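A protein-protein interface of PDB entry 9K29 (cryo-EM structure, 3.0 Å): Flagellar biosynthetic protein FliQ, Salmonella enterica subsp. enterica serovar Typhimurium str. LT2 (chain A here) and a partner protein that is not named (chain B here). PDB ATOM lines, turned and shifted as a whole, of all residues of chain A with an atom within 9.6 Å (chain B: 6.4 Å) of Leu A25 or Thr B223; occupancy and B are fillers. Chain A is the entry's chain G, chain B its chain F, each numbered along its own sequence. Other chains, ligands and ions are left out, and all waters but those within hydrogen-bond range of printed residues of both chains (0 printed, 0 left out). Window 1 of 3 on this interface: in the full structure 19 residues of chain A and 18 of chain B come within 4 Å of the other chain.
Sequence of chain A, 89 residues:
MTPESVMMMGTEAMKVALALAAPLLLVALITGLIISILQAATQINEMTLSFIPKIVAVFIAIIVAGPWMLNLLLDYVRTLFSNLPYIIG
Of chain B, only Pro B219 and Thr B223 come within 4 Å of Leu A25. Of the printed residues of chain A, Thr B223 touches Leu A25 (3.3 Å). Val B224 touches none of the printed residues of chain A. No residue of chain A comes within 4 Å of Gly B225. Ile B226 touches one residue of chain A. Of the printed residues of chain A, Met B227 touches Leu A18. Printed residues of chain B within 4 Å of Leu A29: Leu B220. Of the printed residues of chain B, Leu A18 touches Ile B226 and Met B227. Printed residues of chain A within 4 Å of Leu B220: Leu A29 (3.7 Å). Of the printed residues of chain A, Pro B219 touches Leu A25. Val A27 touches none of the printed residues of chain B. Met B106 touches none of the printed residues of chain A. The nearest printed residue of chain B that does not touch Leu A18 is Thr B223 (4.5 Å).
CG2 of Ile B226 touches CB of Leu A18 (3.8 Å). Leu A18 touches Met B227 (CD2 to CG, 3.9 Å). Pro B219 touches Leu A25 (CB to O, 3.8 Å). OG1 of Thr B223 touches CB of Leu A25 (3.3 Å). CD2 of Leu A29 touches CD1 of Leu B220, at 3.7 Å.
Of the 24 printed residues of chain A, 3 touch a printed residue of chain B. Printed residues of chain A that touch a printed residue of chain B: Leu A18, Leu A25 and Leu A29. Hydrophobic or aromatic side chains of chain A that line the printed part of chain B: Leu A18, Leu A25 and Leu A29. Of the 12 printed residues of chain B, 5 touch a printed residue of chain A. Among the printed residues, 5 pairs touch across the chains. Among the printed residues, no Asp or Glu carboxylate lies within 4 Å of a Lys or Arg side-chain nitrogen of the other chain.
OG1 of Thr B223 sits at hydrogen-bond distance from O of Pro B219 (3.0 Å).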
ATOM      1  N   MET A  14     -14.506  -2.996  11.551  1.00  0.00           N
ATOM      2  CA  MET A  14     -15.147  -1.693  11.689  1.00  0.00           C
ATOM      3  C   MET A  14     -16.555  -1.703  11.109  1.00  0.00           C
ATOM      4  O   MET A  14     -17.443  -1.015  11.621  1.00  0.00           O
ATOM      5  CB  MET A  14     -14.295  -0.610  11.035  1.00  0.00           C
ATOM      6  CG  MET A  14     -12.968  -0.406  11.732  1.00  0.00           C
ATOM      7  SD  MET A  14     -13.179   0.105  13.450  1.00  0.00           S
ATOM      8  CE  MET A  14     -13.837   1.756  13.251  1.00  0.00           C
ATOM      9  N   ALA A  17     -18.632  -3.246  13.805  1.00  0.00           N
ATOM     10  CA  ALA A  17     -18.818  -2.277  14.881  1.00  0.00           C
ATOM     11  C   ALA A  17     -19.849  -1.222  14.502  1.00  0.00           C
ATOM     12  O   ALA A  17     -20.696  -0.849  15.322  1.00  0.00           O
ATOM     13  CB  ALA A  17     -17.485  -1.619  15.234  1.00  0.00           C
ATOM     14  N   LEU A  18     -19.790  -0.727  13.264  1.00  0.00           N
ATOM     15  CA  LEU A  18     -20.778   0.243  12.806  1.00  0.00           C
ATOM     16  C   LEU A  18     -22.175  -0.361  12.785  1.00  0.00           C
ATOM     17  O   LEU A  18     -23.135   0.268  13.242  1.00  0.00           O
ATOM     18  CB  LEU A  18     -20.397   0.761  11.419  1.00  0.00           C
ATOM     19  CG  LEU A  18     -21.399   1.708  10.759  1.00  0.00           C
ATOM     20  CD1 LEU A  18     -21.529   2.991  11.560  1.00  0.00           C
ATOM     21  CD2 LEU A  18     -20.987   2.004   9.328  1.00  0.00           C
ATOM     22  N   ALA A  19     -22.307  -1.586  12.272  1.00  0.00           N
ATOM     23  CA  ALA A  19     -23.614  -2.234  12.236  1.00  0.00           C
ATOM     24  C   ALA A  19     -24.161  -2.469  13.636  1.00  0.00           C
ATOM     25  O   ALA A  19     -25.382  -2.494  13.830  1.00  0.00           O
ATOM     26  CB  ALA A  19     -23.527  -3.554  11.472  1.00  0.00           C
ATOM     27  N   LEU A  20     -23.280  -2.649  14.620  1.00  0.00           N
ATOM     28  CA  LEU A  20     -23.733  -2.814  15.997  1.00  0.00           C
ATOM     29  C   LEU A  20     -24.202  -1.491  16.588  1.00  0.00           C
ATOM     30  O   LEU A  20     -25.212  -1.444  17.299  1.00  0.00           O
ATOM     31  CB  LEU A  20     -22.612  -3.403  16.849  1.00  0.00           C
ATOM     32  CG  LEU A  20     -22.341  -4.901  16.736  1.00  0.00           C
ATOM     33  CD1 LEU A  20     -21.268  -5.302  17.729  1.00  0.00           C
ATOM     34  CD2 LEU A  20     -23.612  -5.693  16.966  1.00  0.00           C
ATOM     35  N   ALA A  21     -23.482  -0.406  16.304  1.00  0.00           N
ATOM     36  CA  ALA A  21     -23.734   0.873  16.953  1.00  0.00           C
ATOM     37  C   ALA A  21     -24.644   1.795  16.157  1.00  0.00           C
ATOM     38  O   ALA A  21     -25.239   2.704  16.745  1.00  0.00           O
ATOM     39  CB  ALA A  21     -22.409   1.590  17.230  1.00  0.00           C
ATOM     40  N   ALA A  22     -24.760   1.596  14.843  1.00  0.00           N
ATOM     41  CA  ALA A  22     -25.616   2.470  14.043  1.00  0.00           C
ATOM     42  C   ALA A  22     -27.065   2.503  14.515  1.00  0.00           C
ATOM     43  O   ALA A  22     -27.627   3.609  14.585  1.00  0.00           O
ATOM     44  CB  ALA A  22     -25.541   2.073  12.563  1.00  0.00           C
ATOM     45  N   PRO A  23     -27.730   1.375  14.840  1.00  0.00           N
ATOM     46  CA  PRO A  23     -29.116   1.468  15.321  1.00  0.00           C
ATOM     47  C   PRO A  23     -29.266   2.335  16.562  1.00  0.00           C
ATOM     48  O   PRO A  23     -30.082   3.260  16.577  1.00  0.00           O
ATOM     49  CB  PRO A  23     -29.481   0.009  15.618  1.00  0.00           C
ATOM     50  CG  PRO A  23     -28.624  -0.775  14.707  1.00  0.00           C
ATOM     51  CD  PRO A  23     -27.324  -0.030  14.650  1.00  0.00           C
ATOM     52  N   LEU A  24     -28.484   2.045  17.603  1.00  0.00           N
ATOM     53  CA  LEU A  24     -28.625   2.771  18.862  1.00  0.00           C
ATOM     54  C   LEU A  24     -28.248   4.240  18.706  1.00  0.00           C
ATOM     55  O   LEU A  24     -28.954   5.127  19.201  1.00  0.00           O
ATOM     56  CB  LEU A  24     -27.777   2.104  19.945  1.00  0.00           C
ATOM     57  CG  LEU A  24     -27.962   0.591  20.077  1.00  0.00           C
ATOM     58  CD1 LEU A  24     -27.120   0.038  21.213  1.00  0.00           C
ATOM     59  CD2 LEU A  24     -29.428   0.250  20.279  1.00  0.00           C
ATOM     60  N   LEU A  25     -27.135   4.516  18.021  1.00  0.00           N
ATOM     61  CA  LEU A  25     -26.717   5.901  17.826  1.00  0.00           C
ATOM     62  C   LEU A  25     -27.743   6.677  17.012  1.00  0.00           C
ATOM     63  O   LEU A  25     -28.067   7.824  17.338  1.00  0.00           O
ATOM     64  CB  LEU A  25     -25.350   5.952  17.146  1.00  0.00           C
ATOM     65  CG  LEU A  25     -24.135   5.507  17.960  1.00  0.00           C
ATOM     66  CD1 LEU A  25     -22.976   5.173  17.038  1.00  0.00           C
ATOM     67  CD2 LEU A  25     -23.733   6.580  18.949  1.00  0.00           C
ATOM     68  N   LEU A  26     -28.267   6.065  15.947  1.00  0.00           N
ATOM     69  CA  LEU A  26     -29.257   6.742  15.118  1.00  0.00           C
ATOM     70  C   LEU A  26     -30.554   6.976  15.882  1.00  0.00           C
ATOM     71  O   LEU A  26     -31.184   8.026  15.729  1.00  0.00           O
ATOM     72  CB  LEU A  26     -29.516   5.937  13.847  1.00  0.00           C
ATOM     73  CG  LEU A  26     -28.511   6.159  12.716  1.00  0.00           C
ATOM     74  CD1 LEU A  26     -28.757   5.184  11.576  1.00  0.00           C
ATOM     75  CD2 LEU A  26     -28.567   7.595  12.223  1.00  0.00           C
ATOM     76  N   VAL A  27     -30.971   6.011  16.704  1.00  0.00           N
ATOM     77  CA  VAL A  27     -32.183   6.190  17.499  1.00  0.00           C
ATOM     78  C   VAL A  27     -31.998   7.320  18.504  1.00  0.00           C
ATOM     79  O   VAL A  27     -32.891   8.159  18.690  1.00  0.00           O
ATOM     80  CB  VAL A  27     -32.568   4.869  18.190  1.00  0.00           C
ATOM     81  CG1 VAL A  27     -33.543   5.122  19.324  1.00  0.00           C
ATOM     82  CG2 VAL A  27     -33.168   3.905  17.182  1.00  0.00           C
ATOM     83  N   ALA A  28     -30.839   7.362  19.167  1.00  0.00           N
ATOM     84  CA  ALA A  28     -30.565   8.448  20.102  1.00  0.00           C
ATOM     85  C   ALA A  28     -30.558   9.794  19.393  1.00  0.00           C
ATOM     86  O   ALA A  28     -31.124  10.772  19.895  1.00  0.00           O
ATOM     87  CB  ALA A  28     -29.235   8.207  20.813  1.00  0.00           C
ATOM     88  N   LEU A  29     -29.935   9.859  18.214  1.00  0.00           N
ATOM     89  CA  LEU A  29     -29.917  11.101  17.449  1.00  0.00           C
ATOM     90  C   LEU A  29     -31.324  11.527  17.052  1.00  0.00           C
ATOM     91  O   LEU A  29     -31.675  12.708  17.153  1.00  0.00           O
ATOM     92  CB  LEU A  29     -29.043  10.931  16.209  1.00  0.00           C
ATOM     93  CG  LEU A  29     -28.872  12.149  15.303  1.00  0.00           C
ATOM     94  CD1 LEU A  29     -28.481  13.375  16.111  1.00  0.00           C
ATOM     95  CD2 LEU A  29     -27.846  11.860  14.222  1.00  0.00           C
ATOM     96  N   ILE A  30     -32.146  10.578  16.602  1.00  0.00           N
ATOM     97  CA  ILE A  30     -33.493  10.902  16.151  1.00  0.00           C
ATOM     98  C   ILE A  30     -34.338  11.412  17.310  1.00  0.00           C
ATOM     99  O   ILE A  30     -35.045  12.419  17.186  1.00  0.00           O
ATOM    100  CB  ILE A  30     -34.139   9.679  15.475  1.00  0.00           C
ATOM    101  CG1 ILE A  30     -33.553   9.473  14.078  1.00  0.00           C
ATOM    102  CG2 ILE A  30     -35.648   9.842  15.397  1.00  0.00           C
ATOM    103  CD1 ILE A  30     -33.617  10.703  13.202  1.00  0.00           C
ATOM    104  N   THR A  31     -34.277  10.733  18.458  1.00  0.00           N
ATOM    105  CA  THR A  31     -35.089  11.170  19.589  1.00  0.00           C
ATOM    106  C   THR A  31     -34.589  12.498  20.151  1.00  0.00           C
ATOM    107  O   THR A  31     -35.394  13.340  20.569  1.00  0.00           O
ATOM    108  CB  THR A  31     -35.141  10.084  20.669  1.00  0.00           C
ATOM    109  OG1 THR A  31     -36.075  10.465  21.687  1.00  0.00           O
ATOM    110  CG2 THR A  31     -33.783   9.849  21.293  1.00  0.00           C
ATOM    111  N   GLY A  32     -33.271  12.723  20.141  1.00  0.00           N
ATOM    112  CA  GLY A  32     -32.757  14.019  20.544  1.00  0.00           C
ATOM    113  C   GLY A  32     -33.219  15.131  19.624  1.00  0.00           C
ATOM    114  O   GLY A  32     -33.604  16.209  20.083  1.00  0.00           O
ATOM    115  N   LEU A  33     -33.198  14.880  18.313  1.00  0.00           N
ATOM    116  CA  LEU A  33     -33.702  15.862  17.358  1.00  0.00           C
ATOM    117  C   LEU A  33     -35.180  16.142  17.583  1.00  0.00           C
ATOM    118  O   LEU A  33     -35.614  17.297  17.533  1.00  0.00           O
ATOM    119  CB  LEU A  33     -33.466  15.376  15.929  1.00  0.00           C
ATOM    120  CG  LEU A  33     -32.251  15.932  15.188  1.00  0.00           C
ATOM    121  CD1 LEU A  33     -32.300  15.538  13.722  1.00  0.00           C
ATOM    122  CD2 LEU A  33     -32.183  17.442  15.337  1.00  0.00           C
ATOM    123  N   LYS A  54     -33.995  10.000  25.536  1.00  0.00           N
ATOM    124  CA  LYS A  54     -32.908   9.307  24.850  1.00  0.00           C
ATOM    125  C   LYS A  54     -32.624   7.957  25.498  1.00  0.00           C
ATOM    126  O   LYS A  54     -32.436   6.951  24.802  1.00  0.00           O
ATOM    127  CB  LYS A  54     -31.650  10.175  24.844  1.00  0.00           C
ATOM    128  CG  LYS A  54     -31.661  11.271  23.794  1.00  0.00           C
ATOM    129  CD  LYS A  54     -30.461  12.190  23.931  1.00  0.00           C
ATOM    130  CE  LYS A  54     -29.187  11.495  23.493  1.00  0.00           C
ATOM    131  NZ  LYS A  54     -28.024  12.423  23.496  1.00  0.00           N
ATOM    132  N   ALA A  57     -35.512   5.603  24.577  1.00  0.00           N
ATOM    133  CA  ALA A  57     -35.441   5.181  23.183  1.00  0.00           C
ATOM    134  C   ALA A  57     -34.321   4.173  22.964  1.00  0.00           C
ATOM    135  O   ALA A  57     -34.501   3.192  22.234  1.00  0.00           O
ATOM    136  CB  ALA A  57     -35.257   6.398  22.279  1.00  0.00           C
ATOM    137  N   VAL A  58     -33.159   4.393  23.583  1.00  0.00           N
ATOM    138  CA  VAL A  58     -32.058   3.447  23.433  1.00  0.00           C
ATOM    139  C   VAL A  58     -32.407   2.114  24.084  1.00  0.00           C
ATOM    140  O   VAL A  58     -32.085   1.046  23.552  1.00  0.00           O
ATOM    141  CB  VAL A  58     -30.760   4.048  24.001  1.00  0.00           C
ATOM    142  CG1 VAL A  58     -29.743   2.958  24.295  1.00  0.00           C
ATOM    143  CG2 VAL A  58     -30.186   5.056  23.021  1.00  0.00           C
ATOM    144  N   ALA A  61     -34.769   0.365  21.707  1.00  0.00           N
ATOM    145  CA  ALA A  61     -34.033  -0.136  20.551  1.00  0.00           C
ATOM    146  C   ALA A  61     -33.214  -1.368  20.910  1.00  0.00           C
ATOM    147  O   ALA A  61     -33.110  -2.308  20.114  1.00  0.00           O
ATOM    148  CB  ALA A  61     -33.133   0.962  19.986  1.00  0.00           C
ATOM    149  N   ILE A  62     -32.617  -1.377  22.104  1.00  0.00           N
ATOM    150  CA  ILE A  62     -31.869  -2.545  22.559  1.00  0.00           C
ATOM    151  C   ILE A  62     -32.793  -3.746  22.690  1.00  0.00           C
ATOM    152  O   ILE A  62     -32.441  -4.865  22.298  1.00  0.00           O
ATOM    153  CB  ILE A  62     -31.148  -2.232  23.884  1.00  0.00           C
ATOM    154  CG1 ILE A  62     -29.871  -1.435  23.620  1.00  0.00           C
ATOM    155  CG2 ILE A  62     -30.829  -3.511  24.642  1.00  0.00           C
ATOM    156  CD1 ILE A  62     -29.075  -1.130  24.867  1.00  0.00           C
ATOM    157  N   MET A  69     -28.513  -7.985  16.651  1.00  0.00           N
ATOM    158  CA  MET A  69     -27.121  -7.645  16.932  1.00  0.00           C
ATOM    159  C   MET A  69     -26.381  -8.826  17.548  1.00  0.00           C
ATOM    160  O   MET A  69     -25.207  -9.065  17.234  1.00  0.00           O
ATOM    161  CB  MET A  69     -27.046  -6.429  17.856  1.00  0.00           C
ATOM    162  CG  MET A  69     -27.552  -5.137  17.235  1.00  0.00           C
ATOM    163  SD  MET A  69     -27.380  -3.717  18.336  1.00  0.00           S
ATOM    164  CE  MET A  69     -28.687  -4.024  19.519  1.00  0.00           C
ATOM    165  N   MET B 106     -13.847  12.405  18.219  1.00  0.00           N
ATOM    166  CA  MET B 106     -15.111  11.683  18.137  1.00  0.00           C
ATOM    167  C   MET B 106     -15.914  11.823  19.424  1.00  0.00           C
ATOM    168  O   MET B 106     -17.147  11.749  19.395  1.00  0.00           O
ATOM    169  CB  MET B 106     -14.852  10.210  17.833  1.00  0.00           C
ATOM    170  CG  MET B 106     -14.900   9.861  16.358  1.00  0.00           C
ATOM    171  SD  MET B 106     -14.511   8.130  16.044  1.00  0.00           S
ATOM    172  CE  MET B 106     -15.334   7.347  17.425  1.00  0.00           C
ATOM    173  N   PHE B 218     -22.876  14.556  19.837  1.00  0.00           N
ATOM    174  CA  PHE B 218     -22.152  13.336  20.194  1.00  0.00           C
ATOM    175  C   PHE B 218     -22.638  12.106  19.435  1.00  0.00           C
ATOM    176  O   PHE B 218     -21.791  11.377  18.892  1.00  0.00           O
ATOM    177  CB  PHE B 218     -22.196  13.136  21.711  1.00  0.00           C
ATOM    178  CG  PHE B 218     -21.329  14.098  22.470  1.00  0.00           C
ATOM    179  CD1 PHE B 218     -20.335  14.814  21.823  1.00  0.00           C
ATOM    180  CD2 PHE B 218     -21.525  14.313  23.821  1.00  0.00           C
ATOM    181  CE1 PHE B 218     -19.537  15.701  22.517  1.00  0.00           C
ATOM    182  CE2 PHE B 218     -20.736  15.209  24.516  1.00  0.00           C
ATOM    183  CZ  PHE B 218     -19.741  15.900  23.865  1.00  0.00           C
ATOM    184  N   PRO B 219     -23.941  11.806  19.347  1.00  0.00           N
ATOM    185  CA  PRO B 219     -24.340  10.640  18.537  1.00  0.00           C
ATOM    186  C   PRO B 219     -23.926  10.758  17.081  1.00  0.00           C
ATOM    187  O   PRO B 219     -23.325   9.825  16.526  1.00  0.00           O
ATOM    188  CB  PRO B 219     -25.866  10.612  18.692  1.00  0.00           C
ATOM    189  CG  PRO B 219     -26.131  11.328  19.960  1.00  0.00           C
ATOM    190  CD  PRO B 219     -25.102  12.411  20.025  1.00  0.00           C
ATOM    191  N   LEU B 220     -24.228  11.892  16.447  1.00  0.00           N
ATOM    192  CA  LEU B 220     -23.896  12.080  15.042  1.00  0.00           C
ATOM    193  C   LEU B 220     -22.388  12.085  14.822  1.00  0.00           C
ATOM    194  O   LEU B 220     -21.898  11.476  13.864  1.00  0.00           O
ATOM    195  CB  LEU B 220     -24.524  13.378  14.530  1.00  0.00           C
ATOM    196  CG  LEU B 220     -24.605  13.605  13.019  1.00  0.00           C
ATOM    197  CD1 LEU B 220     -25.808  14.469  12.685  1.00  0.00           C
ATOM    198  CD2 LEU B 220     -23.343  14.249  12.489  1.00  0.00           C
ATOM    199  N   THR B 221     -21.640  12.767  15.693  1.00  0.00           N
ATOM    200  CA  THR B 221     -20.189  12.800  15.547  1.00  0.00           C
ATOM    201  C   THR B 221     -19.591  11.411  15.710  1.00  0.00           C
ATOM    202  O   THR B 221     -18.684  11.030  14.964  1.00  0.00           O
ATOM    203  CB  THR B 221     -19.568  13.767  16.555  1.00  0.00           C
ATOM    204  OG1 THR B 221     -20.166  15.061  16.405  1.00  0.00           O
ATOM    205  CG2 THR B 221     -18.071  13.885  16.329  1.00  0.00           C
ATOM    206  N   LEU B 222     -20.086  10.635  16.678  1.00  0.00           N
ATOM    207  CA  LEU B 222     -19.581   9.280  16.862  1.00  0.00           C
ATOM    208  C   LEU B 222     -19.884   8.410  15.650  1.00  0.00           C
ATOM    209  O   LEU B 222     -19.024   7.646  15.197  1.00  0.00           O
ATOM    210  CB  LEU B 222     -20.171   8.660  18.128  1.00  0.00           C
ATOM    211  CG  LEU B 222     -19.571   9.125  19.456  1.00  0.00           C
ATOM    212  CD1 LEU B 222     -20.562   8.942  20.595  1.00  0.00           C
ATOM    213  CD2 LEU B 222     -18.276   8.392  19.745  1.00  0.00           C
ATOM    214  N   THR B 223     -21.100   8.512  15.108  1.00  0.00           N
ATOM    215  CA  THR B 223     -21.447   7.718  13.932  1.00  0.00           C
ATOM    216  C   THR B 223     -20.575   8.090  12.737  1.00  0.00           C
ATOM    217  O   THR B 223     -20.059   7.209  12.034  1.00  0.00           O
ATOM    218  CB  THR B 223     -22.926   7.907  13.595  1.00  0.00           C
ATOM    219  OG1 THR B 223     -23.726   7.512  14.715  1.00  0.00           O
ATOM    220  CG2 THR B 223     -23.307   7.063  12.395  1.00  0.00           C
ATOM    221  N   VAL B 224     -20.385   9.390  12.504  1.00  0.00           N
ATOM    222  CA  VAL B 224     -19.561   9.834  11.385  1.00  0.00           C
ATOM    223  C   VAL B 224     -18.115   9.399  11.580  1.00  0.00           C
ATOM    224  O   VAL B 224     -17.448   8.983  10.628  1.00  0.00           O
ATOM    225  CB  VAL B 224     -19.679  11.357  11.203  1.00  0.00           C
ATOM    226  CG1 VAL B 224     -18.703  11.843  10.146  1.00  0.00           C
ATOM    227  CG2 VAL B 224     -21.097  11.730  10.812  1.00  0.00           C
ATOM    228  N   GLY B 225     -17.607   9.484  12.810  1.00  0.00           N
ATOM    229  CA  GLY B 225     -16.245   9.051  13.067  1.00  0.00           C
ATOM    230  C   GLY B 225     -16.056   7.563  12.852  1.00  0.00           C
ATOM    231  O   GLY B 225     -15.033   7.131  12.317  1.00  0.00           O
ATOM    232  N   ILE B 226     -17.035   6.758  13.270  1.00  0.00           N
ATOM    233  CA  ILE B 226     -16.959   5.320  13.030  1.00  0.00           C
ATOM    234  C   ILE B 226     -16.958   5.031  11.534  1.00  0.00           C
ATOM    235  O   ILE B 226     -16.172   4.207  11.048  1.00  0.00           O
ATOM    236  CB  ILE B 226     -18.108   4.591  13.751  1.00  0.00           C
ATOM    237  CG1 ILE B 226     -17.926   4.679  15.267  1.00  0.00           C
ATOM    238  CG2 ILE B 226     -18.181   3.140  13.311  1.00  0.00           C
ATOM    239  CD1 ILE B 226     -19.085   4.114  16.053  1.00  0.00           C
ATOM    240  N   MET B 227     -17.825   5.713  10.779  1.00  0.00           N
ATOM    241  CA  MET B 227     -17.831   5.523   9.329  1.00  0.00           C
ATOM    242  C   MET B 227     -16.497   5.923   8.708  1.00  0.00           C
ATOM    243  O   MET B 227     -15.973   5.218   7.837  1.00  0.00           O
ATOM    244  CB  MET B 227     -18.974   6.313   8.691  1.00  0.00           C
ATOM    245  CG  MET B 227     -20.364   5.813   9.042  1.00  0.00           C
ATOM    246  SD  MET B 227     -21.655   6.800   8.259  1.00  0.00           S
ATOM    247  CE  MET B 227     -23.128   6.036   8.932  1.00  0.00           C
ATOM    248  N   LEU B 228     -15.933   7.052   9.143  1.00  0.00           N
ATOM    249  CA  LEU B 228     -14.663   7.510   8.588  1.00  0.00           C
ATOM    250  C   LEU B 228     -13.536   6.536   8.901  1.00  0.00           C
ATOM    251  O   LEU B 228     -12.709   6.233   8.034  1.00  0.00           O
ATOM    252  CB  LEU B 228     -14.328   8.901   9.121  1.00  0.00           C
ATOM    253  CG  LEU B 228     -15.232  10.043   8.662  1.00  0.00           C
ATOM    254  CD1 LEU B 228     -14.691  11.371   9.150  1.00  0.00           C
ATOM    255  CD2 LEU B 228     -15.367  10.037   7.150  1.00  0.00           C
